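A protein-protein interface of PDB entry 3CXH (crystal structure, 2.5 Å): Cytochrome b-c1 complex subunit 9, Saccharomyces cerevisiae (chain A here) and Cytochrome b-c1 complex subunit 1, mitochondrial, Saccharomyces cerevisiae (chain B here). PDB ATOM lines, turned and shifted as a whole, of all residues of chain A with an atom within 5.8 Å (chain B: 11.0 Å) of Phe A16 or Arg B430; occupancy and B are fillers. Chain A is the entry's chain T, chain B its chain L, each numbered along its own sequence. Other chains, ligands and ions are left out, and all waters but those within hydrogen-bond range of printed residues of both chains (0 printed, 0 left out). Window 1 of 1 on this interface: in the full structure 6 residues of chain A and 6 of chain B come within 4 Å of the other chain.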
ATOM      1  N   ASN A  13      13.320  -5.072 -15.143  1.00  0.00           N
ATOM      2  CA  ASN A  13      14.683  -5.334 -14.707  1.00  0.00           C
ATOM      3  C   ASN A  13      14.982  -6.793 -15.032  1.00  0.00           C
ATOM      4  O   ASN A  13      14.071  -7.620 -15.147  1.00  0.00           O
ATOM      5  CB  ASN A  13      14.825  -5.146 -13.195  1.00  0.00           C
ATOM      6  CG  ASN A  13      15.474  -3.834 -12.825  1.00  0.00           C
ATOM      7  OD1 ASN A  13      15.149  -3.242 -11.796  1.00  0.00           O
ATOM      8  ND2 ASN A  13      16.398  -3.373 -13.654  1.00  0.00           N
ATOM      9  N   ALA A  14      16.259  -7.096 -15.228  1.00  0.00           N
ATOM     10  CA  ALA A  14      16.657  -8.466 -15.486  1.00  0.00           C
ATOM     11  C   ALA A  14      16.749  -9.097 -14.110  1.00  0.00           C
ATOM     12  O   ALA A  14      16.826  -8.388 -13.109  1.00  0.00           O
ATOM     13  CB  ALA A  14      18.005  -8.505 -16.175  1.00  0.00           C
ATOM     14  N   VAL A  15      16.677 -10.420 -14.052  1.00  0.00           N
ATOM     15  CA  VAL A  15      16.783 -11.135 -12.786  1.00  0.00           C
ATOM     16  C   VAL A  15      18.205 -10.969 -12.224  1.00  0.00           C
ATOM     17  O   VAL A  15      19.186 -11.079 -12.954  1.00  0.00           O
ATOM     18  CB  VAL A  15      16.465 -12.624 -12.982  1.00  0.00           C
ATOM     19  CG1 VAL A  15      16.438 -13.325 -11.657  1.00  0.00           C
ATOM     20  CG2 VAL A  15      15.124 -12.777 -13.697  1.00  0.00           C
ATOM     21  N   PHE A  16      18.304 -10.672 -10.934  1.00  0.00           N
ATOM     22  CA  PHE A  16      19.594 -10.468 -10.278  1.00  0.00           C
ATOM     23  C   PHE A  16      20.232 -11.791  -9.878  1.00  0.00           C
ATOM     24  O   PHE A  16      19.522 -12.776  -9.682  1.00  0.00           O
ATOM     25  CB  PHE A  16      19.422  -9.569  -9.042  1.00  0.00           C
ATOM     26  CG  PHE A  16      19.014  -8.145  -9.357  1.00  0.00           C
ATOM     27  CD1 PHE A  16      18.804  -7.235  -8.330  1.00  0.00           C
ATOM     28  CD2 PHE A  16      18.858  -7.710 -10.672  1.00  0.00           C
ATOM     29  CE1 PHE A  16      18.444  -5.906  -8.609  1.00  0.00           C
ATOM     30  CE2 PHE A  16      18.499  -6.390 -10.962  1.00  0.00           C
ATOM     31  CZ  PHE A  16      18.293  -5.489  -9.931  1.00  0.00           C
ATOM     32  N   VAL A  17      21.563 -11.804  -9.736  1.00  0.00           N
ATOM     33  CA  VAL A  17      22.308 -13.022  -9.360  1.00  0.00           C
ATOM     34  C   VAL A  17      21.731 -13.768  -8.171  1.00  0.00           C
ATOM     35  O   VAL A  17      21.480 -14.971  -8.253  1.00  0.00           O
ATOM     36  CB  VAL A  17      23.804 -12.777  -9.017  1.00  0.00           C
ATOM     37  CG1 VAL A  17      24.693 -13.573  -9.961  1.00  0.00           C
ATOM     38  CG2 VAL A  17      24.146 -11.300  -8.999  1.00  0.00           C
ATOM     39  N   GLY A  18      21.557 -13.054  -7.062  1.00  0.00           N
ATOM     40  CA  GLY A  18      21.012 -13.658  -5.858  1.00  0.00           C
ATOM     41  C   GLY A  18      19.786 -14.492  -6.145  1.00  0.00           C
ATOM     42  O   GLY A  18      19.697 -15.650  -5.736  1.00  0.00           O
ATOM     43  N   THR A  19      18.852 -13.916  -6.893  1.00  0.00           N
ATOM     44  CA  THR A  19      17.633 -14.625  -7.241  1.00  0.00           C
ATOM     45  C   THR A  19      17.972 -15.795  -8.155  1.00  0.00           C
ATOM     46  O   THR A  19      17.464 -16.897  -7.953  1.00  0.00           O
ATOM     47  CB  THR A  19      16.611 -13.694  -7.903  1.00  0.00           C
ATOM     48  OG1 THR A  19      16.369 -12.581  -7.035  1.00  0.00           O
ATOM     49  CG2 THR A  19      15.301 -14.427  -8.152  1.00  0.00           C
ATOM     50  N   ILE A  20      18.852 -15.571  -9.128  1.00  0.00           N
ATOM     51  CA  ILE A  20      19.254 -16.643 -10.035  1.00  0.00           C
ATOM     52  C   ILE A  20      19.785 -17.831  -9.224  1.00  0.00           C
ATOM     53  O   ILE A  20      19.282 -18.953  -9.361  1.00  0.00           O
ATOM     54  CB  ILE A  20      20.330 -16.171 -11.043  1.00  0.00           C
ATOM     55  CG1 ILE A  20      19.709 -15.205 -12.057  1.00  0.00           C
ATOM     56  CG2 ILE A  20      20.962 -17.368 -11.763  1.00  0.00           C
ATOM     57  CD1 ILE A  20      18.674 -15.855 -12.947  1.00  0.00           C
ATOM     58  N   PHE A  21      20.757 -17.565  -8.345  1.00  0.00           N
ATOM     59  CA  PHE A  21      21.343 -18.605  -7.498  1.00  0.00           C
ATOM     60  C   PHE A  21      20.270 -19.267  -6.645  1.00  0.00           C
ATOM     61  O   PHE A  21      20.163 -20.491  -6.614  1.00  0.00           O
ATOM     62  CB  PHE A  21      22.438 -18.036  -6.593  1.00  0.00           C
ATOM     63  CG  PHE A  21      23.723 -17.721  -7.307  1.00  0.00           C
ATOM     64  CD1 PHE A  21      23.976 -18.224  -8.579  1.00  0.00           C
ATOM     65  CD2 PHE A  21      24.686 -16.924  -6.700  1.00  0.00           C
ATOM     66  CE1 PHE A  21      25.168 -17.939  -9.238  1.00  0.00           C
ATOM     67  CE2 PHE A  21      25.882 -16.632  -7.349  1.00  0.00           C
ATOM     68  CZ  PHE A  21      26.124 -17.142  -8.623  1.00  0.00           C
ATOM     69  N   LYS B 323      28.449   5.805 -17.369  1.00  0.00           N
ATOM     70  CA  LYS B 323      28.604   5.288 -16.016  1.00  0.00           C
ATOM     71  C   LYS B 323      28.264   6.362 -15.006  1.00  0.00           C
ATOM     72  O   LYS B 323      27.745   6.058 -13.934  1.00  0.00           O
ATOM     73  CB  LYS B 323      29.982   4.675 -15.774  1.00  0.00           C
ATOM     74  CG  LYS B 323      30.034   3.220 -16.166  1.00  0.00           C
ATOM     75  CD  LYS B 323      29.172   2.406 -15.232  1.00  0.00           C
ATOM     76  CE  LYS B 323      28.852   0.995 -15.751  1.00  0.00           C
ATOM     77  NZ  LYS B 323      27.813   1.015 -16.813  1.00  0.00           N
ATOM     78  N   ASN B 326      24.423   6.527 -14.694  1.00  0.00           N
ATOM     79  CA  ASN B 326      23.865   5.463 -13.845  1.00  0.00           C
ATOM     80  C   ASN B 326      23.732   5.976 -12.425  1.00  0.00           C
ATOM     81  O   ASN B 326      22.796   5.624 -11.702  1.00  0.00           O
ATOM     82  CB  ASN B 326      24.779   4.235 -13.780  1.00  0.00           C
ATOM     83  CG  ASN B 326      25.076   3.631 -15.134  1.00  0.00           C
ATOM     84  OD1 ASN B 326      26.122   3.014 -15.314  1.00  0.00           O
ATOM     85  ND2 ASN B 326      24.157   3.784 -16.085  1.00  0.00           N
ATOM     86  N   ARG B 327      24.694   6.805 -12.029  1.00  0.00           N
ATOM     87  CA  ARG B 327      24.709   7.371 -10.694  1.00  0.00           C
ATOM     88  C   ARG B 327      23.453   8.161 -10.358  1.00  0.00           C
ATOM     89  O   ARG B 327      23.035   8.194  -9.202  1.00  0.00           O
ATOM     90  CB  ARG B 327      25.957   8.220 -10.502  1.00  0.00           C
ATOM     91  CG  ARG B 327      27.253   7.402 -10.522  1.00  0.00           C
ATOM     92  CD  ARG B 327      28.443   8.246 -10.098  1.00  0.00           C
ATOM     93  NE  ARG B 327      28.184   8.891  -8.817  1.00  0.00           N
ATOM     94  CZ  ARG B 327      28.045  10.202  -8.663  1.00  0.00           C
ATOM     95  NH1 ARG B 327      27.794  10.705  -7.463  1.00  0.00           N
ATOM     96  NH2 ARG B 327      28.175  11.010  -9.706  1.00  0.00           N
ATOM     97  N   THR B 329      20.572   7.359 -10.839  1.00  0.00           N
ATOM     98  CA  THR B 329      19.567   6.422 -10.348  1.00  0.00           C
ATOM     99  C   THR B 329      19.923   5.833  -8.987  1.00  0.00           C
ATOM    100  O   THR B 329      19.042   5.602  -8.145  1.00  0.00           O
ATOM    101  CB  THR B 329      19.387   5.239 -11.336  1.00  0.00           C
ATOM    102  OG1 THR B 329      18.813   5.711 -12.556  1.00  0.00           O
ATOM    103  CG2 THR B 329      18.500   4.151 -10.747  1.00  0.00           C
ATOM    104  N   ILE B 330      21.216   5.613  -8.756  1.00  0.00           N
ATOM    105  CA  ILE B 330      21.642   4.978  -7.513  1.00  0.00           C
ATOM    106  C   ILE B 330      22.478   5.729  -6.483  1.00  0.00           C
ATOM    107  O   ILE B 330      22.413   5.390  -5.304  1.00  0.00           O
ATOM    108  CB  ILE B 330      22.373   3.644  -7.812  1.00  0.00           C
ATOM    109  CG1 ILE B 330      23.648   3.924  -8.611  1.00  0.00           C
ATOM    110  CG2 ILE B 330      21.448   2.689  -8.575  1.00  0.00           C
ATOM    111  CD1 ILE B 330      24.532   2.718  -8.799  1.00  0.00           C
ATOM    112  N   SER B 331      23.235   6.748  -6.882  1.00  0.00           N
ATOM    113  CA  SER B 331      24.080   7.420  -5.902  1.00  0.00           C
ATOM    114  C   SER B 331      24.292   8.919  -5.976  1.00  0.00           C
ATOM    115  O   SER B 331      25.142   9.425  -5.247  1.00  0.00           O
ATOM    116  CB  SER B 331      25.447   6.757  -5.892  1.00  0.00           C
ATOM    117  OG  SER B 331      26.095   6.965  -7.135  1.00  0.00           O
ATOM    118  N   LYS B 393      16.500  10.653  -8.526  1.00  0.00           N
ATOM    119  CA  LYS B 393      16.624   9.196  -8.639  1.00  0.00           C
ATOM    120  C   LYS B 393      15.396   8.544  -9.257  1.00  0.00           C
ATOM    121  O   LYS B 393      15.528   7.658 -10.102  1.00  0.00           O
ATOM    122  CB  LYS B 393      16.894   8.533  -7.291  1.00  0.00           C
ATOM    123  CG  LYS B 393      18.260   8.786  -6.701  1.00  0.00           C
ATOM    124  CD  LYS B 393      18.420   8.031  -5.384  1.00  0.00           C
ATOM    125  CE  LYS B 393      19.787   8.294  -4.761  1.00  0.00           C
ATOM    126  NZ  LYS B 393      19.996   7.514  -3.508  1.00  0.00           N
ATOM    127  N   TRP B 401      17.929   4.538 -16.465  1.00  0.00           N
ATOM    128  CA  TRP B 401      18.293   3.165 -16.129  1.00  0.00           C
ATOM    129  C   TRP B 401      17.775   2.078 -17.060  1.00  0.00           C
ATOM    130  O   TRP B 401      16.576   1.756 -17.067  1.00  0.00           O
ATOM    131  CB  TRP B 401      17.877   2.831 -14.694  1.00  0.00           C
ATOM    132  CG  TRP B 401      18.522   1.569 -14.169  1.00  0.00           C
ATOM    133  CD1 TRP B 401      18.020   0.301 -14.235  1.00  0.00           C
ATOM    134  CD2 TRP B 401      19.790   1.466 -13.510  1.00  0.00           C
ATOM    135  NE1 TRP B 401      18.894  -0.584 -13.662  1.00  0.00           N
ATOM    136  CE2 TRP B 401      19.992   0.102 -13.207  1.00  0.00           C
ATOM    137  CE3 TRP B 401      20.778   2.393 -13.151  1.00  0.00           C
ATOM    138  CZ2 TRP B 401      21.151  -0.366 -12.557  1.00  0.00           C
ATOM    139  CZ3 TRP B 401      21.930   1.932 -12.506  1.00  0.00           C
ATOM    140  CH2 TRP B 401      22.105   0.560 -12.217  1.00  0.00           C
ATOM    141  N   ASP B 402      18.696   1.497 -17.827  1.00  0.00           N
ATOM    142  CA  ASP B 402      18.374   0.409 -18.733  1.00  0.00           C
ATOM    143  C   ASP B 402      17.285   0.793 -19.730  1.00  0.00           C
ATOM    144  O   ASP B 402      16.351   0.043 -19.961  1.00  0.00           O
ATOM    145  CB  ASP B 402      17.981  -0.837 -17.907  1.00  0.00           C
ATOM    146  CG  ASP B 402      17.849  -2.104 -18.745  1.00  0.00           C
ATOM    147  OD1 ASP B 402      18.572  -2.251 -19.751  1.00  0.00           O
ATOM    148  OD2 ASP B 402      17.022  -2.975 -18.384  1.00  0.00           O
ATOM    149  N   SER B 424      24.310  -1.409 -23.239  1.00  0.00           N
ATOM    150  CA  SER B 424      24.613  -2.154 -22.012  1.00  0.00           C
ATOM    151  C   SER B 424      24.992  -1.227 -20.848  1.00  0.00           C
ATOM    152  O   SER B 424      24.527  -1.412 -19.723  1.00  0.00           O
ATOM    153  CB  SER B 424      25.760  -3.147 -22.250  1.00  0.00           C
ATOM    154  OG  SER B 424      25.378  -4.185 -23.146  1.00  0.00           O
ATOM    155  N   MET B 426      23.930   1.405 -19.889  1.00  0.00           N
ATOM    156  CA  MET B 426      22.848   2.224 -19.339  1.00  0.00           C
ATOM    157  C   MET B 426      22.415   1.706 -17.957  1.00  0.00           C
ATOM    158  O   MET B 426      21.529   2.273 -17.309  1.00  0.00           O
ATOM    159  CB  MET B 426      21.656   2.300 -20.303  1.00  0.00           C
ATOM    160  CG  MET B 426      21.928   3.038 -21.617  1.00  0.00           C
ATOM    161  SD  MET B 426      22.425   4.794 -21.455  1.00  0.00           S
ATOM    162  CE  MET B 426      20.928   5.500 -20.662  1.00  0.00           C
ATOM    163  N   SER B 427      23.050   0.627 -17.510  1.00  0.00           N
ATOM    164  CA  SER B 427      22.774   0.059 -16.195  1.00  0.00           C
ATOM    165  C   SER B 427      24.052  -0.587 -15.661  1.00  0.00           C
ATOM    166  O   SER B 427      25.061  -0.632 -16.363  1.00  0.00           O
ATOM    167  CB  SER B 427      21.642  -0.971 -16.257  1.00  0.00           C
ATOM    168  OG  SER B 427      22.008  -2.100 -17.022  1.00  0.00           O
ATOM    169  N   MET B 428      24.008  -1.060 -14.419  1.00  0.00           N
ATOM    170  CA  MET B 428      25.151  -1.708 -13.780  1.00  0.00           C
ATOM    171  C   MET B 428      24.743  -3.058 -13.230  1.00  0.00           C
ATOM    172  O   MET B 428      23.564  -3.313 -13.015  1.00  0.00           O
ATOM    173  CB  MET B 428      25.646  -0.878 -12.602  1.00  0.00           C
ATOM    174  CG  MET B 428      26.053   0.520 -12.941  1.00  0.00           C
ATOM    175  SD  MET B 428      26.233   1.445 -11.424  1.00  0.00           S
ATOM    176  CE  MET B 428      28.022   1.411 -11.257  1.00  0.00           C
ATOM    177  N   MET B 429      25.727  -3.912 -12.977  1.00  0.00           N
ATOM    178  CA  MET B 429      25.481  -5.226 -12.405  1.00  0.00           C
ATOM    179  C   MET B 429      25.276  -5.040 -10.904  1.00  0.00           C
ATOM    180  O   MET B 429      25.840  -4.121 -10.309  1.00  0.00           O
ATOM    181  CB  MET B 429      26.704  -6.122 -12.614  1.00  0.00           C
ATOM    182  CG  MET B 429      27.125  -6.317 -14.062  1.00  0.00           C
ATOM    183  SD  MET B 429      25.984  -7.366 -14.949  1.00  0.00           S
ATOM    184  CE  MET B 429      26.363  -8.996 -14.271  1.00  0.00           C
ATOM    185  N   ARG B 430      24.469  -5.897 -10.291  1.00  0.00           N
ATOM    186  CA  ARG B 430      24.248  -5.824  -8.848  1.00  0.00           C
ATOM    187  C   ARG B 430      23.769  -7.159  -8.288  1.00  0.00           C
ATOM    188  O   ARG B 430      23.364  -8.041  -9.042  1.00  0.00           O
ATOM    189  CB  ARG B 430      23.279  -4.688  -8.499  1.00  0.00           C
ATOM    190  CG  ARG B 430      21.818  -4.952  -8.791  1.00  0.00           C
ATOM    191  CD  ARG B 430      21.068  -3.645  -9.050  1.00  0.00           C
ATOM    192  NE  ARG B 430      21.279  -2.601  -8.037  1.00  0.00           N
ATOM    193  CZ  ARG B 430      20.555  -2.445  -6.924  1.00  0.00           C
ATOM    194  NH1 ARG B 430      20.836  -1.448  -6.092  1.00  0.00           N
ATOM    195  NH2 ARG B 430      19.573  -3.296  -6.620  1.00  0.00           N
ATOM    196  N   TRP B 431      23.852  -7.326  -6.974  1.00  0.00           N
ATOM    197  CA  TRP B 431      23.426  -8.574  -6.348  1.00  0.00           C
ATOM    198  C   TRP B 431      21.898  -8.650  -6.180  1.00  0.00           C
ATOM    199  O   TRP B 431      21.332  -9.755  -6.362  1.00  0.00           O
ATOM    200  CB  TRP B 431      24.142  -8.771  -5.000  1.00  0.00           C
ATOM    201  CG  TRP B 431      24.018 -10.175  -4.444  1.00  0.00           C
ATOM    202  CD1 TRP B 431      23.042 -10.645  -3.603  1.00  0.00           C
ATOM    203  CD2 TRP B 431      24.877 -11.293  -4.719  1.00  0.00           C
ATOM    204  NE1 TRP B 431      23.237 -11.984  -3.347  1.00  0.00           N
ATOM    205  CE2 TRP B 431      24.353 -12.407  -4.018  1.00  0.00           C
ATOM    206  CE3 TRP B 431      26.037 -11.462  -5.491  1.00  0.00           C
ATOM    207  CZ2 TRP B 431      24.949 -13.673  -4.069  1.00  0.00           C
ATOM    208  CZ3 TRP B 431      26.629 -12.723  -5.542  1.00  0.00           C
ATOM    209  CH2 TRP B 431      26.082 -13.811  -4.833  1.00  0.00           C
ATOM    210  OXT TRP B 431      21.276  -7.601  -5.885  1.00  0.00           O
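Asn A13 touches just one residue of chain B: Trp B401.
Phe A16 touches just these residues of chain B: Arg B430 and Trp B431.
Val A17 touches two residues of chain B.
Of chain B, only Trp B431 comes within 4 Å of Gly A18.
Thr A19 touches none of the printed residues of chain B.
Printed residues of chain B within 4 Å of Phe A21: Trp B431 (3.8 Å).
Lys B323 touches none of the printed residues of chain A.
Of the printed residues of chain A, Trp B431 touches Phe A16, Val A17, Gly A18 and Phe A21.
The nearest residue of chain B that does not touch Phe A16 is Trp B401 (6.2 Å).
The nearest residue of chain A that does not touch Arg B430 is Gly A18 (5.7 Å).
The nearest printed residue of chain B that does not touch Phe A21 is Arg B430 (9.1 Å).
The chain-end carboxylate (O) of Trp B431 sits at hydrogen-bond distance from the backbone NH (N) of Gly A18 (3.4 Å).
Of the 9 printed residues of chain A, 5 touch a printed residue of chain B.
Hydrophobic or aromatic side chains of chain A that line the printed part of chain B: Phe A16, Val A17 and Phe A21.
Of the 16 printed residues of chain B, 3 touch a printed residue of chain A.
Printed residues of chain B that touch a printed residue of chain A: Trp B401, Arg B430 and Trp B431.
Hydrophobic or aromatic side chains of chain B that line the printed part of chain A: Trp B401 and Trp B431.
Along chain B the printed residues that touch a printed residue of chain A span positions 401 to 431.
Among the printed residues, 7 pairs touch across the chains.
Among the printed residues, no Asp or Glu carboxylate lies within 4 Å of a Lys or Arg side-chain nitrogen of the other chain.
NE1 of Trp B401 touches ND2 of Asn A13, at 3.7 Å.
Arg B430 touches Phe A16 (CD to CZ, 3.4 Å).
CB of Phe A16 touches O of Trp B431 (3.3 Å).
CG2 of Val A17 touches O of Arg B430, 3.4 Å away.
Val A17 touches Trp B431 (CG2 to CA, 3.9 Å).
Trp B431 touches Phe A21 (CH2 to CE2, 3.8 Å).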
